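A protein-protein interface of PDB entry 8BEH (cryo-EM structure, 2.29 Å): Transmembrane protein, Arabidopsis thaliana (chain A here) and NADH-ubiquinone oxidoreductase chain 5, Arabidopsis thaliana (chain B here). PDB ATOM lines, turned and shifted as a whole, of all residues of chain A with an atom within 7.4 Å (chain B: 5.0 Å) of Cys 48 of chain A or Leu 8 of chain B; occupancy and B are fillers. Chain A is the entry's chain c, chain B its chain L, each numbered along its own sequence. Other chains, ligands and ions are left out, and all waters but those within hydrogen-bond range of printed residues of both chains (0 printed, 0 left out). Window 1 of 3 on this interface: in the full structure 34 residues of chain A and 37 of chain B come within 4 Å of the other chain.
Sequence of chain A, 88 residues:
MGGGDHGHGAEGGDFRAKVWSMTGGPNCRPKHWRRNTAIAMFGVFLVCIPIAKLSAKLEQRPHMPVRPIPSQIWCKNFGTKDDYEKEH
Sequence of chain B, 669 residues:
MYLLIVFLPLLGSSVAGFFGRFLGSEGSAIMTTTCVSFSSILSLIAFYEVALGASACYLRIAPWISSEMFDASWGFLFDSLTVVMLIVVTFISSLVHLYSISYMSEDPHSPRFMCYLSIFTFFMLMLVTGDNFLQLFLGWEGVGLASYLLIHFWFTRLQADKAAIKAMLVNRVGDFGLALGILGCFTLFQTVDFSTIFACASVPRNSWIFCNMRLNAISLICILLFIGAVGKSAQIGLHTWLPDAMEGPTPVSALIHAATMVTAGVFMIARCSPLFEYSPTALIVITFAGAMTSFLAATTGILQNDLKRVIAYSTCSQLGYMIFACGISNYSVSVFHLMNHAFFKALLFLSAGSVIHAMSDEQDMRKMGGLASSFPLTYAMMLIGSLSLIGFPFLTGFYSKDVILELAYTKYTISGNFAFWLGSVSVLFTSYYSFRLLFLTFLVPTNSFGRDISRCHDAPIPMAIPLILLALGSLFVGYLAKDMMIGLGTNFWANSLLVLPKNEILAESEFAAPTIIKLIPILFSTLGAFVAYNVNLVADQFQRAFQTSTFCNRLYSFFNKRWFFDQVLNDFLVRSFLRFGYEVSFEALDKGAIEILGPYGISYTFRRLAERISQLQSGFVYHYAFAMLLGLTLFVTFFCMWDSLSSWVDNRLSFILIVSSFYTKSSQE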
ATOM      1  N   PHE A  42      -5.651  11.223  17.139  1.00  0.00           N
ATOM      2  CA  PHE A  42      -6.725  12.196  17.005  1.00  0.00           C
ATOM      3  C   PHE A  42      -7.475  12.008  15.690  1.00  0.00           C
ATOM      4  O   PHE A  42      -8.709  12.110  15.647  1.00  0.00           O
ATOM      5  CB  PHE A  42      -6.155  13.608  17.125  1.00  0.00           C
ATOM      6  CG  PHE A  42      -7.195  14.673  17.158  1.00  0.00           C
ATOM      7  CD1 PHE A  42      -7.275  15.612  16.149  1.00  0.00           C
ATOM      8  CD2 PHE A  42      -8.114  14.722  18.189  1.00  0.00           C
ATOM      9  CE1 PHE A  42      -8.236  16.590  16.181  1.00  0.00           C
ATOM     10  CE2 PHE A  42      -9.079  15.695  18.220  1.00  0.00           C
ATOM     11  CZ  PHE A  42      -9.143  16.630  17.214  1.00  0.00           C
ATOM     12  N   GLY A  43      -6.746  11.717  14.610  1.00  0.00           N
ATOM     13  CA  GLY A  43      -7.400  11.447  13.342  1.00  0.00           C
ATOM     14  C   GLY A  43      -8.299  10.224  13.387  1.00  0.00           C
ATOM     15  O   GLY A  43      -9.420  10.250  12.876  1.00  0.00           O
ATOM     16  N   VAL A  44      -7.823   9.117  13.973  1.00  0.00           N
ATOM     17  CA  VAL A  44      -8.638   7.889  14.056  1.00  0.00           C
ATOM     18  C   VAL A  44      -9.916   8.210  14.899  1.00  0.00           C
ATOM     19  O   VAL A  44     -10.973   7.927  14.383  1.00  0.00           O
ATOM     20  CB  VAL A  44      -7.823   6.650  14.512  1.00  0.00           C
ATOM     21  CG1 VAL A  44      -8.689   5.596  15.190  1.00  0.00           C
ATOM     22  CG2 VAL A  44      -6.936   6.063  13.433  1.00  0.00           C
ATOM     23  N   PHE A  45      -9.806   8.969  16.013  1.00  0.00           N
ATOM     24  CA  PHE A  45     -10.996   9.285  16.802  1.00  0.00           C
ATOM     25  C   PHE A  45     -11.993  10.131  16.005  1.00  0.00           C
ATOM     26  O   PHE A  45     -13.212   9.870  16.024  1.00  0.00           O
ATOM     27  CB  PHE A  45     -10.580   9.990  18.093  1.00  0.00           C
ATOM     28  CG  PHE A  45     -11.709  10.657  18.811  1.00  0.00           C
ATOM     29  CD1 PHE A  45     -11.892  12.025  18.724  1.00  0.00           C
ATOM     30  CD2 PHE A  45     -12.597   9.914  19.568  1.00  0.00           C
ATOM     31  CE1 PHE A  45     -12.931  12.636  19.381  1.00  0.00           C
ATOM     32  CE2 PHE A  45     -13.639  10.523  20.225  1.00  0.00           C
ATOM     33  CZ  PHE A  45     -13.806  11.886  20.132  1.00  0.00           C
ATOM     34  N   LEU A  46     -11.493  11.140  15.283  1.00  0.00           N
ATOM     35  CA  LEU A  46     -12.380  11.959  14.465  1.00  0.00           C
ATOM     36  C   LEU A  46     -13.080  11.130  13.401  1.00  0.00           C
ATOM     37  O   LEU A  46     -14.280  11.298  13.167  1.00  0.00           O
ATOM     38  CB  LEU A  46     -11.611  13.101  13.816  1.00  0.00           C
ATOM     39  CG  LEU A  46     -11.165  14.200  14.765  1.00  0.00           C
ATOM     40  CD1 LEU A  46     -10.482  15.290  13.971  1.00  0.00           C
ATOM     41  CD2 LEU A  46     -12.356  14.729  15.550  1.00  0.00           C
ATOM     42  N   VAL A  47     -12.347  10.231  12.741  1.00  0.00           N
ATOM     43  CA  VAL A  47     -12.961   9.356  11.748  1.00  0.00           C
ATOM     44  C   VAL A  47     -13.975   8.425  12.400  1.00  0.00           C
ATOM     45  O   VAL A  47     -14.977   8.050  11.780  1.00  0.00           O
ATOM     46  CB  VAL A  47     -11.869   8.574  10.989  1.00  0.00           C
ATOM     47  CG1 VAL A  47     -12.478   7.613   9.986  1.00  0.00           C
ATOM     48  CG2 VAL A  47     -10.942   9.537  10.278  1.00  0.00           C
ATOM     49  N   CYS A  48     -13.746   8.049  13.658  1.00  0.00           N
ATOM     50  CA  CYS A  48     -14.631   7.101  14.325  1.00  0.00           C
ATOM     51  C   CYS A  48     -15.961   7.730  14.712  1.00  0.00           C
ATOM     52  O   CYS A  48     -16.959   7.014  14.850  1.00  0.00           O
ATOM     53  CB  CYS A  48     -13.949   6.524  15.563  1.00  0.00           C
ATOM     54  SG  CYS A  48     -12.847   5.152  15.219  1.00  0.00           S
ATOM     55  N   ILE A  49     -15.994   9.043  14.923  1.00  0.00           N
ATOM     56  CA  ILE A  49     -17.261   9.684  15.305  1.00  0.00           C
ATOM     57  C   ILE A  49     -18.371   9.442  14.275  1.00  0.00           C
ATOM     58  O   ILE A  49     -19.442   8.924  14.647  1.00  0.00           O
ATOM     59  CB  ILE A  49     -17.071  11.190  15.564  1.00  0.00           C
ATOM     60  CG1 ILE A  49     -16.335  11.422  16.884  1.00  0.00           C
ATOM     61  CG2 ILE A  49     -18.406  11.920  15.546  1.00  0.00           C
ATOM     62  CD1 ILE A  49     -15.430  12.614  16.863  1.00  0.00           C
ATOM     63  N   PRO A  50     -18.191   9.776  12.986  1.00  0.00           N
ATOM     64  CA  PRO A  50     -19.273   9.510  12.023  1.00  0.00           C
ATOM     65  C   PRO A  50     -19.605   8.039  11.874  1.00  0.00           C
ATOM     66  O   PRO A  50     -20.773   7.699  11.643  1.00  0.00           O
ATOM     67  CB  PRO A  50     -18.727  10.095  10.710  1.00  0.00           C
ATOM     68  CG  PRO A  50     -17.665  11.027  11.121  1.00  0.00           C
ATOM     69  CD  PRO A  50     -17.044  10.407  12.311  1.00  0.00           C
ATOM     70  N   ILE A  51     -18.612   7.157  11.991  1.00  0.00           N
ATOM     71  CA  ILE A  51     -18.887   5.726  11.921  1.00  0.00           C
ATOM     72  C   ILE A  51     -19.809   5.312  13.058  1.00  0.00           C
ATOM     73  O   ILE A  51     -20.753   4.541  12.859  1.00  0.00           O
ATOM     74  CB  ILE A  51     -17.573   4.921  11.936  1.00  0.00           C
ATOM     75  CG1 ILE A  51     -16.788   5.134  10.642  1.00  0.00           C
ATOM     76  CG2 ILE A  51     -17.852   3.441  12.129  1.00  0.00           C
ATOM     77  CD1 ILE A  51     -15.432   4.456  10.645  1.00  0.00           C
ATOM     78  N   ALA A  52     -19.550   5.819  14.265  1.00  0.00           N
ATOM     79  CA  ALA A  52     -20.404   5.499  15.403  1.00  0.00           C
ATOM     80  C   ALA A  52     -21.818   6.031  15.202  1.00  0.00           C
ATOM     81  O   ALA A  52     -22.795   5.343  15.518  1.00  0.00           O
ATOM     82  CB  ALA A  52     -19.795   6.050  16.691  1.00  0.00           C
ATOM     83  N   LYS A  53     -21.947   7.250  14.670  1.00  0.00           N
ATOM     84  CA  LYS A  53     -23.278   7.799  14.414  1.00  0.00           C
ATOM     85  C   LYS A  53     -24.043   6.952  13.401  1.00  0.00           C
ATOM     86  O   LYS A  53     -25.226   6.636  13.599  1.00  0.00           O
ATOM     87  CB  LYS A  53     -23.167   9.243  13.926  1.00  0.00           C
ATOM     88  CG  LYS A  53     -22.813  10.234  15.011  1.00  0.00           C
ATOM     89  CD  LYS A  53     -22.716  11.642  14.465  1.00  0.00           C
ATOM     90  CE  LYS A  53     -23.462  12.623  15.350  1.00  0.00           C
ATOM     91  NZ  LYS A  53     -24.833  12.893  14.840  1.00  0.00           N
ATOM     92  N   LEU A  54     -23.378   6.565  12.309  1.00  0.00           N
ATOM     93  CA  LEU A  54     -24.037   5.751  11.294  1.00  0.00           C
ATOM     94  C   LEU A  54     -24.412   4.382  11.847  1.00  0.00           C
ATOM     95  O   LEU A  54     -25.490   3.856  11.544  1.00  0.00           O
ATOM     96  CB  LEU A  54     -23.143   5.610  10.062  1.00  0.00           C
ATOM     97  CG  LEU A  54     -23.617   4.608   9.008  1.00  0.00           C
ATOM     98  CD1 LEU A  54     -24.818   5.153   8.261  1.00  0.00           C
ATOM     99  CD2 LEU A  54     -22.496   4.243   8.040  1.00  0.00           C
ATOM    100  N   LEU B   3     -20.421  -1.085  14.347  1.00  0.00           N
ATOM    101  CA  LEU B   3     -19.547  -0.850  13.203  1.00  0.00           C
ATOM    102  C   LEU B   3     -18.113  -0.588  13.652  1.00  0.00           C
ATOM    103  O   LEU B   3     -17.157  -0.983  12.971  1.00  0.00           O
ATOM    104  CB  LEU B   3     -20.078   0.321  12.385  1.00  0.00           C
ATOM    105  CG  LEU B   3     -21.193   0.014  11.387  1.00  0.00           C
ATOM    106  CD1 LEU B   3     -21.493   1.230  10.537  1.00  0.00           C
ATOM    107  CD2 LEU B   3     -20.843  -1.182  10.530  1.00  0.00           C
ATOM    108  N   LEU B   4     -17.950   0.083  14.796  1.00  0.00           N
ATOM    109  CA  LEU B   4     -16.616   0.364  15.316  1.00  0.00           C
ATOM    110  C   LEU B   4     -15.852  -0.923  15.582  1.00  0.00           C
ATOM    111  O   LEU B   4     -14.655  -1.009  15.291  1.00  0.00           O
ATOM    112  CB  LEU B   4     -16.705   1.209  16.588  1.00  0.00           C
ATOM    113  CG  LEU B   4     -17.201   2.651  16.468  1.00  0.00           C
ATOM    114  CD1 LEU B   4     -17.235   3.319  17.829  1.00  0.00           C
ATOM    115  CD2 LEU B   4     -16.335   3.455  15.502  1.00  0.00           C
ATOM    116  N   ILE B   5     -16.541  -1.948  16.092  1.00  0.00           N
ATOM    117  CA  ILE B   5     -15.902  -3.235  16.360  1.00  0.00           C
ATOM    118  C   ILE B   5     -15.232  -3.761  15.098  1.00  0.00           C
ATOM    119  O   ILE B   5     -14.075  -4.193  15.117  1.00  0.00           O
ATOM    120  CB  ILE B   5     -16.935  -4.244  16.889  1.00  0.00           C
ATOM    121  CG1 ILE B   5     -17.262  -3.993  18.359  1.00  0.00           C
ATOM    122  CG2 ILE B   5     -16.434  -5.667  16.713  1.00  0.00           C
ATOM    123  CD1 ILE B   5     -18.206  -5.019  18.925  1.00  0.00           C
ATOM    124  N   VAL B   6     -15.959  -3.734  13.984  1.00  0.00           N
ATOM    125  CA  VAL B   6     -15.453  -4.324  12.753  1.00  0.00           C
ATOM    126  C   VAL B   6     -14.367  -3.449  12.136  1.00  0.00           C
ATOM    127  O   VAL B   6     -13.339  -3.955  11.678  1.00  0.00           O
ATOM    128  CB  VAL B   6     -16.613  -4.580  11.773  1.00  0.00           C
ATOM    129  CG1 VAL B   6     -16.087  -5.082  10.434  1.00  0.00           C
ATOM    130  CG2 VAL B   6     -17.599  -5.573  12.367  1.00  0.00           C
ATOM    131  N   PHE B   7     -14.561  -2.129  12.133  1.00  0.00           N
ATOM    132  CA  PHE B   7     -13.719  -1.261  11.319  1.00  0.00           C
ATOM    133  C   PHE B   7     -12.539  -0.633  12.056  1.00  0.00           C
ATOM    134  O   PHE B   7     -11.661  -0.072  11.397  1.00  0.00           O
ATOM    135  CB  PHE B   7     -14.571  -0.157  10.677  1.00  0.00           C
ATOM    136  CG  PHE B   7     -15.457  -0.652   9.567  1.00  0.00           C
ATOM    137  CD1 PHE B   7     -14.929  -0.967   8.326  1.00  0.00           C
ATOM    138  CD2 PHE B   7     -16.816  -0.821   9.770  1.00  0.00           C
ATOM    139  CE1 PHE B   7     -15.739  -1.427   7.305  1.00  0.00           C
ATOM    140  CE2 PHE B   7     -17.633  -1.283   8.753  1.00  0.00           C
ATOM    141  CZ  PHE B   7     -17.093  -1.587   7.521  1.00  0.00           C
ATOM    142  N   LEU B   8     -12.471  -0.724  13.387  1.00  0.00           N
ATOM    143  CA  LEU B   8     -11.318  -0.176  14.102  1.00  0.00           C
ATOM    144  C   LEU B   8      -9.996  -0.829  13.699  1.00  0.00           C
ATOM    145  O   LEU B   8      -9.021  -0.093  13.453  1.00  0.00           O
ATOM    146  CB  LEU B   8     -11.566  -0.278  15.611  1.00  0.00           C
ATOM    147  CG  LEU B   8     -12.109   0.983  16.290  1.00  0.00           C
ATOM    148  CD1 LEU B   8     -12.374   0.730  17.763  1.00  0.00           C
ATOM    149  CD2 LEU B   8     -11.145   2.140  16.108  1.00  0.00           C
ATOM    150  N   PRO B   9      -9.878  -2.162  13.617  1.00  0.00           N
ATOM    151  CA  PRO B   9      -8.612  -2.739  13.133  1.00  0.00           C
ATOM    152  C   PRO B   9      -8.260  -2.324  11.716  1.00  0.00           C
ATOM    153  O   PRO B   9      -7.073  -2.183  11.408  1.00  0.00           O
ATOM    154  CB  PRO B   9      -8.838  -4.255  13.242  1.00  0.00           C
ATOM    155  CG  PRO B   9     -10.061  -4.432  14.037  1.00  0.00           C
ATOM    156  CD  PRO B   9     -10.870  -3.204  13.936  1.00  0.00           C
ATOM    157  N   LEU B  10      -9.252  -2.121  10.846  1.00  0.00           N
ATOM    158  CA  LEU B  10      -8.967  -1.595   9.514  1.00  0.00           C
ATOM    159  C   LEU B  10      -8.342  -0.210   9.595  1.00  0.00           C
ATOM    160  O   LEU B  10      -7.378   0.083   8.884  1.00  0.00           O
ATOM    161  CB  LEU B  10     -10.244  -1.557   8.673  1.00  0.00           C
ATOM    162  CG  LEU B  10     -10.133  -1.043   7.230  1.00  0.00           C
ATOM    163  CD1 LEU B  10      -9.011  -1.727   6.454  1.00  0.00           C
ATOM    164  CD2 LEU B  10     -11.454  -1.164   6.500  1.00  0.00           C
ATOM    165  N   LEU B  11      -8.875   0.653  10.464  1.00  0.00           N
ATOM    166  CA  LEU B  11      -8.314   1.990  10.632  1.00  0.00           C
ATOM    167  C   LEU B  11      -6.876   1.922  11.131  1.00  0.00           C
ATOM    168  O   LEU B  11      -5.992   2.626  10.622  1.00  0.00           O
ATOM    169  CB  LEU B  11      -9.178   2.797  11.600  1.00  0.00           C
ATOM    170  CG  LEU B  11     -10.494   3.335  11.045  1.00  0.00           C
ATOM    171  CD1 LEU B  11     -11.326   3.953  12.150  1.00  0.00           C
ATOM    172  CD2 LEU B  11     -10.241   4.335   9.935  1.00  0.00           C
ATOM    173  N   GLY B  12      -6.625   1.072  12.130  1.00  0.00           N
ATOM    174  CA  GLY B  12      -5.272   0.931  12.638  1.00  0.00           C
ATOM    175  C   GLY B  12      -4.304   0.418  11.590  1.00  0.00           C
ATOM    176  O   GLY B  12      -3.193   0.939  11.445  1.00  0.00           O
ATOM    177  N   CYS B  35      -6.095   0.425  18.622  1.00  0.00           N
ATOM    178  CA  CYS B  35      -7.281   0.164  17.804  1.00  0.00           C
ATOM    179  C   CYS B  35      -7.809  -1.274  18.024  1.00  0.00           C
ATOM    180  O   CYS B  35      -9.022  -1.362  18.212  1.00  0.00           O
ATOM    181  CB  CYS B  35      -7.111   0.544  16.318  1.00  0.00           C
ATOM    182  SG  CYS B  35      -6.684   2.257  15.961  1.00  0.00           S
ATOM    183  N   PHE B  38      -9.270  -1.499  21.661  1.00  0.00           N
ATOM    184  CA  PHE B  38     -10.559  -0.828  21.769  1.00  0.00           C
ATOM    185  C   PHE B  38     -11.662  -1.659  21.132  1.00  0.00           C
ATOM    186  O   PHE B  38     -12.778  -1.744  21.663  1.00  0.00           O
ATOM    187  CB  PHE B  38     -10.484   0.557  21.136  1.00  0.00           C
ATOM    188  CG  PHE B  38     -10.250   1.648  22.124  1.00  0.00           C
ATOM    189  CD1 PHE B  38     -11.244   2.019  23.009  1.00  0.00           C
ATOM    190  CD2 PHE B  38      -9.027   2.290  22.191  1.00  0.00           C
ATOM    191  CE1 PHE B  38     -11.030   3.019  23.927  1.00  0.00           C
ATOM    192  CE2 PHE B  38      -8.807   3.287  23.106  1.00  0.00           C
ATOM    193  CZ  PHE B  38      -9.810   3.655  23.975  1.00  0.00           C
ATOM    194  N   SER B  39     -11.363  -2.285  19.990  1.00  0.00           N
ATOM    195  CA  SER B  39     -12.322  -3.200  19.387  1.00  0.00           C
ATOM    196  C   SER B  39     -12.632  -4.365  20.325  1.00  0.00           C
ATOM    197  O   SER B  39     -13.774  -4.822  20.400  1.00  0.00           O
ATOM    198  CB  SER B  39     -11.792  -3.699  18.043  1.00  0.00           C
ATOM    199  OG  SER B  39     -12.268  -4.991  17.745  1.00  0.00           O
ATOM    200  N   LEU B  42     -15.036  -3.089  23.076  1.00  0.00           N
ATOM    201  CA  LEU B  42     -16.378  -2.999  22.520  1.00  0.00           C
ATOM    202  C   LEU B  42     -16.969  -4.380  22.270  1.00  0.00           C
ATOM    203  O   LEU B  42     -18.182  -4.564  22.384  1.00  0.00           O
ATOM    204  CB  LEU B  42     -16.361  -2.181  21.228  1.00  0.00           C
ATOM    205  CG  LEU B  42     -15.860  -0.737  21.272  1.00  0.00           C
ATOM    206  CD1 LEU B  42     -16.047  -0.083  19.915  1.00  0.00           C
ATOM    207  CD2 LEU B  42     -16.543   0.073  22.361  1.00  0.00           C
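O of Val 44 of chain A lies within hydrogen-bond range of SG of Cys 48 of chain A.
Among the printed residues, merely in contact across the chains: Val 44 of chain A with Cys 35 of chain B, Val 47 of chain A with Leu 11 of chain B, Cys 48 of chain A with Leu 4 of chain B, Cys 48 of chain A with Leu 8 of chain B, Cys 48 of chain A with Leu 11 of chain B, Ile 51 of chain A with Leu 3 of chain B, Ile 51 of chain A with Leu 4 of chain B and Ala 52 of chain A with Leu 4 of chain B.
Of the printed residues of chain B, Cys 48 of chain A touches Leu 4, Leu 8 and Leu 11.
Leu 8 of chain B touches just one residue of chain A: Cys 48 (3.6 Å).
Printed residues of chain A within 4 Å of Leu 3 of chain B: Ile 51 (3.8 Å).
Of the printed residues of chain A, Leu 11 of chain B touches Val 47 and Cys 48.
Of the printed residues of chain B, Val 44 of chain A touches Cys 35.
Of the printed residues of chain A, Cys 35 of chain B touches Val 44 (3.97 Å).
Val 6 of chain B touches none of the printed residues of chain A.
Ile 49 of chain A touches none of the printed residues of chain B.
The nearest residue of chain A that does not touch Leu 8 of chain B is Val 44 of chain A (4.3 Å).
Of the 13 printed residues of chain A, 5 touch a printed residue of chain B.
Along chain A the printed residues that touch a printed residue of chain B span positions 44 to 52.
Of the 14 printed residues of chain B, 5 touch a printed residue of chain A.
Hydrophobic or aromatic side chains of chain B that line the printed part of chain A: Leu 3, Leu 4, Leu 8 and Leu 11.
Among the printed residues, 8 pairs touch across the chains.
Among the printed residues, no Asp or Glu carboxylate lies within 4 Å of a Lys or Arg side-chain nitrogen of the other chain.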
